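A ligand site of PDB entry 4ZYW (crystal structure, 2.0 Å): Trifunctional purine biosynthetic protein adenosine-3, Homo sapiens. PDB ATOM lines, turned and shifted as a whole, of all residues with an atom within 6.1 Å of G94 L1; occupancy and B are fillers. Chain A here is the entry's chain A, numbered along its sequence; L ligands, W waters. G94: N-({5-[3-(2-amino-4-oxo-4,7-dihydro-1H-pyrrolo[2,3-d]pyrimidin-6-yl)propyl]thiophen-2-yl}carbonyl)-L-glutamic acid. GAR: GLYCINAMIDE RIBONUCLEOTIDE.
The guanidinium group of Arg 65 is in salt-bridge range of an oxygen (O24) of G94 L1 (2.7 Å). The backbone carbonyl oxygen (O) of Ala 141 is in hydrogen-bond range of a nitrogen (N11) of G94 L1. N of Asp 145 sits at hydrogen-bond distance from O10 of G94 L1, 2.9 Å away. A nitrogen (N5) of G94 L1 lies within hydrogen-bond range of the backbone carbonyl oxygen (O) of Arg 91 (2.9 Å). The guanidinium group (NE) of Arg 91 lies within salt-bridge range of an oxygen (O24) of G94 L1 (3.6 Å). O24 of G94 L1 sits at hydrogen-bond distance from N of Ile 92 (3.0 Å). The backbone NH (N) of Leu 93 is in hydrogen-bond range of a nitrogen (N1) of G94 L1 (3.1 Å). A nitrogen (N11) of G94 L1 sits at hydrogen-bond distance from the backbone carbonyl oxygen of Leu 93, at 3.1 Å. The backbone carbonyl oxygen (O) of Glu 142 lies within hydrogen-bond range of a nitrogen (N11) of G94 L1, at 3.1 Å. OG of Ser 119 is in hydrogen-bond range of O18 of G94 L1, 3.5 Å away.
The guanidinium group (NH1) of Arg 65 sits at hydrogen-bond distance from the backbone carbonyl oxygen (O) of Ile 92, at 2.8 Å. The side-chain carboxylate of Asp 145 sits at hydrogen-bond distance from the backbone NH of Gly 118. The guanidinium group (NH1) of Arg 91 sits close to a ring nitrogen (NE2) of His 59, at 3.3 Å. The backbone carbonyl oxygen (O) of His 138 sits at hydrogen-bond distance from the backbone NH (N) of Asn 107, 2.9 Å away.
S12 of G94 L1 sits close to O of Met 90 (3.6 Å). Residues that only touch G94 L1: Leu 86 (3.9 Å), Phe 89 (3.0 Å), Val 98 (3.6 Å), Asn 107 (3.7 Å), His 138 (3.5 Å), Val 140 (3.4 Å), Asp 143 (3.8 Å) and Val 144 (3.5 Å). Hydrophobic or aromatic side chains within 4 Å of G94 L1: Leu 86, Met 90, Ile 92, Leu 93, Val 98, His 138 and Val 140. Within 4 Å of G94 L1: Arg 65, Leu 86, Phe 89, Met 90, Arg 91, Ile 92, Leu 93, Val 98, Asn 107, Ser 119, His 138, Val 140, Ala 141, Glu 142, Asp 143, Val 144 and Asp 145. The nearest printed residue that does not touch G94 L1 is Gly 118 (4.2 Å).
Water W2 lies within hydrogen-bond range of the side-chain amide oxygen (OD1) of Asn 107 (2.7 Å) and the backbone carbonyl oxygen (O) of Phe 89 (2.8 Å).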
ATOM      1  N   HIS A  59     -30.115  22.025 -27.408  1.00  0.00           N
ATOM      2  CA  HIS A  59     -29.662  21.622 -26.082  1.00  0.00           C
ATOM      3  C   HIS A  59     -28.968  22.756 -25.326  1.00  0.00           C
ATOM      4  O   HIS A  59     -28.939  22.766 -24.100  1.00  0.00           O
ATOM      5  CB  HIS A  59     -28.712  20.424 -26.182  1.00  0.00           C
ATOM      6  CG  HIS A  59     -27.449  20.712 -26.939  1.00  0.00           C
ATOM      7  ND1 HIS A  59     -27.362  20.570 -28.309  1.00  0.00           N
ATOM      8  CD2 HIS A  59     -26.232  21.128 -26.519  1.00  0.00           C
ATOM      9  CE1 HIS A  59     -26.140  20.891 -28.698  1.00  0.00           C
ATOM     10  NE2 HIS A  59     -25.435  21.240 -27.634  1.00  0.00           N
ATOM     11  N   ARG A  65     -29.313  18.229 -18.710  1.00  0.00           N
ATOM     12  CA  ARG A  65     -29.648  17.150 -19.636  1.00  0.00           C
ATOM     13  C   ARG A  65     -31.122  16.726 -19.509  1.00  0.00           C
ATOM     14  O   ARG A  65     -31.795  16.498 -20.522  1.00  0.00           O
ATOM     15  CB  ARG A  65     -28.725  15.955 -19.394  1.00  0.00           C
ATOM     16  CG  ARG A  65     -28.533  15.052 -20.597  1.00  0.00           C
ATOM     17  CD  ARG A  65     -27.375  14.083 -20.406  1.00  0.00           C
ATOM     18  NE  ARG A  65     -26.067  14.752 -20.333  1.00  0.00           N
ATOM     19  CZ  ARG A  65     -25.264  14.954 -21.382  1.00  0.00           C
ATOM     20  NH1 ARG A  65     -25.618  14.542 -22.588  1.00  0.00           N
ATOM     21  NH2 ARG A  65     -24.097  15.565 -21.206  1.00  0.00           N
ATOM     22  N   LEU A  86     -32.343   7.135 -33.234  1.00  0.00           N
ATOM     23  CA  LEU A  86     -31.243   8.099 -33.179  1.00  0.00           C
ATOM     24  C   LEU A  86     -30.399   7.927 -34.448  1.00  0.00           C
ATOM     25  O   LEU A  86     -29.767   6.890 -34.637  1.00  0.00           O
ATOM     26  CB  LEU A  86     -30.397   7.916 -31.915  1.00  0.00           C
ATOM     27  CG  LEU A  86     -31.147   7.896 -30.567  1.00  0.00           C
ATOM     28  CD1 LEU A  86     -30.206   7.994 -29.401  1.00  0.00           C
ATOM     29  CD2 LEU A  86     -32.208   8.996 -30.504  1.00  0.00           C
ATOM     30  N   PHE A  89     -27.654  11.397 -34.258  1.00  0.00           N
ATOM     31  CA  PHE A  89     -27.939  12.234 -33.094  1.00  0.00           C
ATOM     32  C   PHE A  89     -26.778  12.153 -32.119  1.00  0.00           C
ATOM     33  O   PHE A  89     -26.511  11.088 -31.568  1.00  0.00           O
ATOM     34  CB  PHE A  89     -29.246  11.791 -32.427  1.00  0.00           C
ATOM     35  CG  PHE A  89     -29.683  12.672 -31.273  1.00  0.00           C
ATOM     36  CD1 PHE A  89     -30.268  13.909 -31.507  1.00  0.00           C
ATOM     37  CD2 PHE A  89     -29.532  12.241 -29.964  1.00  0.00           C
ATOM     38  CE1 PHE A  89     -30.683  14.709 -30.455  1.00  0.00           C
ATOM     39  CE2 PHE A  89     -29.941  13.035 -28.906  1.00  0.00           C
ATOM     40  CZ  PHE A  89     -30.526  14.272 -29.140  1.00  0.00           C
ATOM     41  N   MET A  90     -26.075  13.251 -31.910  1.00  0.00           N
ATOM     42  CA  MET A  90     -24.860  13.193 -31.105  1.00  0.00           C
ATOM     43  C   MET A  90     -25.028  13.769 -29.712  1.00  0.00           C
ATOM     44  O   MET A  90     -24.207  14.591 -29.288  1.00  0.00           O
ATOM     45  CB  MET A  90     -23.714  13.927 -31.825  1.00  0.00           C
ATOM     46  CG  MET A  90     -23.413  13.395 -33.225  1.00  0.00           C
ATOM     47  SD  MET A  90     -22.978  11.625 -33.278  1.00  0.00           S
ATOM     48  CE  MET A  90     -21.302  11.672 -32.630  1.00  0.00           C
ATOM     49  N   ARG A  91     -26.068  13.365 -28.983  1.00  0.00           N
ATOM     50  CA  ARG A  91     -26.170  13.724 -27.574  1.00  0.00           C
ATOM     51  C   ARG A  91     -26.390  12.477 -26.724  1.00  0.00           C
ATOM     52  O   ARG A  91     -27.054  11.536 -27.165  1.00  0.00           O
ATOM     53  CB  ARG A  91     -27.311  14.714 -27.312  1.00  0.00           C
ATOM     54  CG  ARG A  91     -27.252  15.996 -28.121  1.00  0.00           C
ATOM     55  CD  ARG A  91     -26.185  16.929 -27.595  1.00  0.00           C
ATOM     56  NE  ARG A  91     -26.302  17.159 -26.159  1.00  0.00           N
ATOM     57  CZ  ARG A  91     -25.467  17.918 -25.465  1.00  0.00           C
ATOM     58  NH1 ARG A  91     -24.461  18.522 -26.083  1.00  0.00           N
ATOM     59  NH2 ARG A  91     -25.636  18.082 -24.163  1.00  0.00           N
ATOM     60  N   ILE A  92     -25.843  12.476 -25.514  1.00  0.00           N
ATOM     61  CA  ILE A  92     -26.090  11.403 -24.570  1.00  0.00           C
ATOM     62  C   ILE A  92     -27.399  11.658 -23.822  1.00  0.00           C
ATOM     63  O   ILE A  92     -27.581  12.724 -23.246  1.00  0.00           O
ATOM     64  CB  ILE A  92     -24.943  11.267 -23.583  1.00  0.00           C
ATOM     65  CG1 ILE A  92     -23.683  10.796 -24.321  1.00  0.00           C
ATOM     66  CG2 ILE A  92     -25.311  10.319 -22.461  1.00  0.00           C
ATOM     67  CD1 ILE A  92     -22.428  10.858 -23.475  1.00  0.00           C
ATOM     68  N   LEU A  93     -28.306  10.680 -23.826  1.00  0.00           N
ATOM     69  CA  LEU A  93     -29.603  10.832 -23.173  1.00  0.00           C
ATOM     70  C   LEU A  93     -29.580  10.444 -21.691  1.00  0.00           C
ATOM     71  O   LEU A  93     -28.816   9.564 -21.289  1.00  0.00           O
ATOM     72  CB  LEU A  93     -30.641   9.985 -23.904  1.00  0.00           C
ATOM     73  CG  LEU A  93     -30.837  10.411 -25.364  1.00  0.00           C
ATOM     74  CD1 LEU A  93     -31.462   9.291 -26.142  1.00  0.00           C
ATOM     75  CD2 LEU A  93     -31.703  11.662 -25.419  1.00  0.00           C
ATOM     76  N   SER A  94     -30.426  11.074 -20.888  1.00  0.00           N
ATOM     77  CA  SER A  94     -30.487  10.800 -19.451  1.00  0.00           C
ATOM     78  C   SER A  94     -31.151   9.476 -19.109  1.00  0.00           C
ATOM     79  O   SER A  94     -31.942   8.917 -19.894  1.00  0.00           O
ATOM     80  CB  SER A  94     -31.232  11.925 -18.715  1.00  0.00           C
ATOM     81  OG  SER A  94     -32.630  11.851 -18.960  1.00  0.00           O
ATOM     82  N   GLY A  95     -30.823   8.986 -17.914  1.00  0.00           N
ATOM     83  CA  GLY A  95     -31.370   7.733 -17.397  1.00  0.00           C
ATOM     84  C   GLY A  95     -32.877   7.577 -17.473  1.00  0.00           C
ATOM     85  O   GLY A  95     -33.345   6.608 -18.055  1.00  0.00           O
ATOM     86  N   VAL A  98     -34.164   7.368 -21.047  1.00  0.00           N
ATOM     87  CA  VAL A  98     -33.832   6.064 -21.609  1.00  0.00           C
ATOM     88  C   VAL A  98     -34.737   4.974 -21.033  1.00  0.00           C
ATOM     89  O   VAL A  98     -35.247   4.119 -21.754  1.00  0.00           O
ATOM     90  CB  VAL A  98     -32.348   5.706 -21.374  1.00  0.00           C
ATOM     91  CG1 VAL A  98     -32.068   4.245 -21.760  1.00  0.00           C
ATOM     92  CG2 VAL A  98     -31.446   6.643 -22.164  1.00  0.00           C
ATOM     93  N   ASN A 107     -30.445   3.039 -31.917  1.00  0.00           N
ATOM     94  CA  ASN A 107     -29.328   3.880 -32.311  1.00  0.00           C
ATOM     95  C   ASN A 107     -28.482   3.175 -33.361  1.00  0.00           C
ATOM     96  O   ASN A 107     -28.318   1.961 -33.284  1.00  0.00           O
ATOM     97  CB  ASN A 107     -28.451   4.226 -31.095  1.00  0.00           C
ATOM     98  CG  ASN A 107     -27.251   5.104 -31.451  1.00  0.00           C
ATOM     99  OD1 ASN A 107     -27.422   6.187 -32.013  1.00  0.00           O
ATOM    100  ND2 ASN A 107     -26.056   4.645 -31.108  1.00  0.00           N
ATOM    101  N   GLY A 118     -18.222   5.358 -28.581  1.00  0.00           N
ATOM    102  CA  GLY A 118     -17.963   6.780 -28.486  1.00  0.00           C
ATOM    103  C   GLY A 118     -18.203   7.539 -29.781  1.00  0.00           C
ATOM    104  O   GLY A 118     -18.748   6.978 -30.731  1.00  0.00           O
ATOM    105  N   SER A 119     -17.786   8.801 -29.830  1.00  0.00           N
ATOM    106  CA  SER A 119     -18.149   9.669 -30.945  1.00  0.00           C
ATOM    107  C   SER A 119     -17.181   9.660 -32.127  1.00  0.00           C
ATOM    108  O   SER A 119     -17.485  10.248 -33.180  1.00  0.00           O
ATOM    109  CB  SER A 119     -18.303  11.108 -30.448  1.00  0.00           C
ATOM    110  OG  SER A 119     -17.044  11.609 -30.023  1.00  0.00           O
ATOM    111  N   HIS A 138     -28.520  -0.908 -32.280  1.00  0.00           N
ATOM    112  CA  HIS A 138     -28.802  -1.476 -30.976  1.00  0.00           C
ATOM    113  C   HIS A 138     -29.903  -0.716 -30.271  1.00  0.00           C
ATOM    114  O   HIS A 138     -30.134   0.464 -30.555  1.00  0.00           O
ATOM    115  CB  HIS A 138     -27.533  -1.466 -30.108  1.00  0.00           C
ATOM    116  CG  HIS A 138     -26.984  -0.093 -29.853  1.00  0.00           C
ATOM    117  ND1 HIS A 138     -27.276   0.624 -28.714  1.00  0.00           N
ATOM    118  CD2 HIS A 138     -26.180   0.696 -30.604  1.00  0.00           C
ATOM    119  CE1 HIS A 138     -26.666   1.800 -28.766  1.00  0.00           C
ATOM    120  NE2 HIS A 138     -25.986   1.864 -29.896  1.00  0.00           N
ATOM    121  N   PHE A 139     -30.587  -1.387 -29.335  1.00  0.00           N
ATOM    122  CA  PHE A 139     -31.447  -0.684 -28.395  1.00  0.00           C
ATOM    123  C   PHE A 139     -30.613   0.226 -27.500  1.00  0.00           C
ATOM    124  O   PHE A 139     -29.497  -0.115 -27.081  1.00  0.00           O
ATOM    125  CB  PHE A 139     -32.248  -1.675 -27.534  1.00  0.00           C
ATOM    126  CG  PHE A 139     -33.404  -2.311 -28.266  1.00  0.00           C
ATOM    127  CD1 PHE A 139     -34.527  -1.557 -28.583  1.00  0.00           C
ATOM    128  CD2 PHE A 139     -33.365  -3.640 -28.641  1.00  0.00           C
ATOM    129  CE1 PHE A 139     -35.609  -2.132 -29.244  1.00  0.00           C
ATOM    130  CE2 PHE A 139     -34.427  -4.236 -29.310  1.00  0.00           C
ATOM    131  CZ  PHE A 139     -35.559  -3.472 -29.608  1.00  0.00           C
ATOM    132  N   VAL A 140     -31.158   1.388 -27.189  1.00  0.00           N
ATOM    133  CA  VAL A 140     -30.454   2.350 -26.352  1.00  0.00           C
ATOM    134  C   VAL A 140     -30.690   2.024 -24.875  1.00  0.00           C
ATOM    135  O   VAL A 140     -31.832   2.011 -24.402  1.00  0.00           O
ATOM    136  CB  VAL A 140     -30.912   3.793 -26.651  1.00  0.00           C
ATOM    137  CG1 VAL A 140     -30.268   4.774 -25.683  1.00  0.00           C
ATOM    138  CG2 VAL A 140     -30.580   4.131 -28.092  1.00  0.00           C
ATOM    139  N   ALA A 141     -29.610   1.713 -24.182  1.00  0.00           N
ATOM    140  CA  ALA A 141     -29.627   1.547 -22.735  1.00  0.00           C
ATOM    141  C   ALA A 141     -28.914   2.754 -22.117  1.00  0.00           C
ATOM    142  O   ALA A 141     -28.423   3.614 -22.844  1.00  0.00           O
ATOM    143  CB  ALA A 141     -28.967   0.240 -22.318  1.00  0.00           C
ATOM    144  N   GLU A 142     -28.880   2.818 -20.791  1.00  0.00           N
ATOM    145  CA  GLU A 142     -28.309   3.971 -20.116  1.00  0.00           C
ATOM    146  C   GLU A 142     -26.815   4.092 -20.423  1.00  0.00           C
ATOM    147  O   GLU A 142     -26.340   5.167 -20.802  1.00  0.00           O
ATOM    148  CB  GLU A 142     -28.556   3.883 -18.619  1.00  0.00           C
ATOM    149  CG  GLU A 142     -28.211   5.156 -17.891  1.00  0.00           C
ATOM    150  CD  GLU A 142     -28.868   5.251 -16.524  1.00  0.00           C
ATOM    151  OE1 GLU A 142     -29.896   4.570 -16.305  1.00  0.00           O
ATOM    152  OE2 GLU A 142     -28.347   6.011 -15.683  1.00  0.00           O
ATOM    153  N   ASP A 143     -26.067   3.000 -20.248  1.00  0.00           N
ATOM    154  CA  ASP A 143     -24.665   2.990 -20.643  1.00  0.00           C
ATOM    155  C   ASP A 143     -24.549   3.118 -22.159  1.00  0.00           C
ATOM    156  O   ASP A 143     -25.112   2.328 -22.917  1.00  0.00           O
ATOM    157  CB  ASP A 143     -23.968   1.718 -20.160  1.00  0.00           C
ATOM    158  CG  ASP A 143     -23.665   1.740 -18.680  1.00  0.00           C
ATOM    159  OD1 ASP A 143     -23.727   2.832 -18.081  1.00  0.00           O
ATOM    160  OD2 ASP A 143     -23.364   0.666 -18.120  1.00  0.00           O
ATOM    161  N   VAL A 144     -23.806   4.134 -22.590  1.00  0.00           N
ATOM    162  CA  VAL A 144     -23.693   4.471 -24.001  1.00  0.00           C
ATOM    163  C   VAL A 144     -23.092   3.334 -24.845  1.00  0.00           C
ATOM    164  O   VAL A 144     -22.079   2.740 -24.467  1.00  0.00           O
ATOM    165  CB  VAL A 144     -22.847   5.757 -24.185  1.00  0.00           C
ATOM    166  CG1 VAL A 144     -22.635   6.062 -25.658  1.00  0.00           C
ATOM    167  CG2 VAL A 144     -23.530   6.919 -23.509  1.00  0.00           C
ATOM    168  N   ASP A 145     -23.767   3.005 -25.955  1.00  0.00           N
ATOM    169  CA  ASP A 145     -23.310   2.001 -26.921  1.00  0.00           C
ATOM    170  C   ASP A 145     -23.193   0.615 -26.307  1.00  0.00           C
ATOM    171  O   ASP A 145     -22.424  -0.225 -26.789  1.00  0.00           O
ATOM    172  CB  ASP A 145     -21.974   2.429 -27.545  1.00  0.00           C
ATOM    173  CG  ASP A 145     -22.066   3.730 -28.338  1.00  0.00           C
ATOM    174  OD1 ASP A 145     -23.169   4.087 -28.841  1.00  0.00           O
ATOM    175  OD2 ASP A 145     -21.027   4.408 -28.484  1.00  0.00           O
ATOM    176  N   ALA A 146     -23.959   0.351 -25.253  1.00  0.00           N
ATOM    177  CA  ALA A 146     -23.909  -0.935 -24.559  1.00  0.00           C
ATOM    178  C   ALA A 146     -25.241  -1.687 -24.568  1.00  0.00           C
ATOM    179  O   ALA A 146     -25.319  -2.813 -24.089  1.00  0.00           O
ATOM    180  CB  ALA A 146     -23.445  -0.728 -23.095  1.00  0.00           C
ATOM    181  N   GLY A 147     -26.294  -1.077 -25.115  1.00  0.00           N
ATOM    182  CA  GLY A 147     -27.593  -1.724 -25.194  1.00  0.00           C
ATOM    183  C   GLY A 147     -27.621  -2.925 -26.138  1.00  0.00           C
ATOM    184  O   GLY A 147     -26.658  -3.164 -26.866  1.00  0.00           O
HETATM  185  N1  G94 L   1     -27.453   7.870 -24.840  1.00  0.00           N
HETATM  186  C2  G94 L   1     -27.507   6.835 -24.019  1.00  0.00           C
HETATM  187  N3  G94 L   1     -27.198   5.591 -24.430  1.00  0.00           N
HETATM  188  C4  G94 L   1     -26.786   5.337 -25.688  1.00  0.00           C
HETATM  189  N5  G94 L   1     -26.928   8.613 -27.101  1.00  0.00           N
HETATM  190  C6  G94 L   1     -26.502   8.015 -28.209  1.00  0.00           C
HETATM  191  C7  G94 L   1     -26.333   6.618 -27.970  1.00  0.00           C
HETATM  192  C8  G94 L   1     -26.707   6.433 -26.594  1.00  0.00           C
HETATM  193  C9  G94 L   1     -27.063   7.726 -26.121  1.00  0.00           C
HETATM  194  O10 G94 L   1     -26.447   4.000 -26.065  1.00  0.00           O
HETATM  195  N11 G94 L   1     -27.915   7.005 -22.694  1.00  0.00           N
HETATM  196  S12 G94 L   1     -22.579  11.502 -28.384  1.00  0.00           S
HETATM  197  C13 G94 L   1     -20.957  11.720 -27.861  1.00  0.00           C
HETATM  198  C14 G94 L   1     -20.488  10.411 -27.564  1.00  0.00           C
HETATM  199  C15 G94 L   1     -21.446   9.345 -27.777  1.00  0.00           C
HETATM  200  C16 G94 L   1     -22.700   9.822 -28.251  1.00  0.00           C
HETATM  201  C17 G94 L   1     -19.994  12.944 -27.688  1.00  0.00           C
HETATM  202  O18 G94 L   1     -18.852  12.678 -27.257  1.00  0.00           O
HETATM  203  N19 G94 L   1     -20.185  14.356 -27.958  1.00  0.00           N
HETATM  204  C20 G94 L   1     -21.339  15.061 -28.449  1.00  0.00           C
HETATM  205  C21 G94 L   1     -21.709  16.050 -27.395  1.00  0.00           C
HETATM  206  C22 G94 L   1     -23.063  15.778 -26.755  1.00  0.00           C
HETATM  207  C23 G94 L   1     -23.063  14.756 -25.596  1.00  0.00           C
HETATM  208  O24 G94 L   1     -24.049  14.724 -24.764  1.00  0.00           O
HETATM  209  O25 G94 L   1     -22.073  13.908 -25.461  1.00  0.00           O
HETATM  210  C26 G94 L   1     -20.950  15.852 -29.711  1.00  0.00           C
HETATM  211  O27 G94 L   1     -20.885  15.271 -30.884  1.00  0.00           O
HETATM  212  O28 G94 L   1     -20.705  17.106 -29.610  1.00  0.00           O
HETATM  213  C29 G94 L   1     -26.229   8.742 -29.555  1.00  0.00           C
HETATM  214  C30 G94 L   1     -24.859   9.519 -29.541  1.00  0.00           C
HETATM  215  C31 G94 L   1     -23.869   8.908 -28.551  1.00  0.00           C
HETATM  216  C1  GAR L   2     -23.312   8.002 -39.043  1.00  0.00           C
HETATM  217  O6  GAR L   2     -22.096   7.411 -39.543  1.00  0.00           O
HETATM  218  C2  GAR L   2     -23.633   7.393 -37.688  1.00  0.00           C
HETATM  219  O8  GAR L   2     -23.317   5.997 -37.581  1.00  0.00           O
HETATM  220  C3  GAR L   2     -22.792   8.228 -36.735  1.00  0.00           C
HETATM  221  O4  GAR L   2     -22.883   9.539 -37.276  1.00  0.00           O
HETATM  222  C5  GAR L   2     -23.103   9.481 -38.702  1.00  0.00           C
HETATM  223  C10 GAR L   2     -24.311  10.350 -39.063  1.00  0.00           C
HETATM  224  O12 GAR L   2     -24.443  10.501 -40.477  1.00  0.00           O
HETATM  225  N19 GAR L   2     -23.312   8.155 -35.379  1.00  0.00           N
HETATM  226  C21 GAR L   2     -22.504   8.119 -34.313  1.00  0.00           C
HETATM  227  O22 GAR L   2     -21.278   8.247 -34.393  1.00  0.00           O
HETATM  228  C23 GAR L   2     -23.202   7.920 -32.986  1.00  0.00           C
HETATM  229  N24 GAR L   2     -22.286   8.074 -31.860  1.00  0.00           N
HETATM  230  P15 GAR L   2     -25.847  10.989 -41.150  1.00  0.00           P
HETATM  231  O16 GAR L   2     -26.827   9.885 -40.773  1.00  0.00           O
HETATM  232  O17 GAR L   2     -25.550  11.116 -42.626  1.00  0.00           O
HETATM  233  O18 GAR L   2     -26.181  12.329 -40.498  1.00  0.00           O
HETATM  234  O   HOH W   1     -26.803   1.790 -25.035  1.00  0.00           O
HETATM  235  O   HOH W   2     -27.355   8.735 -32.814  1.00  0.00           O
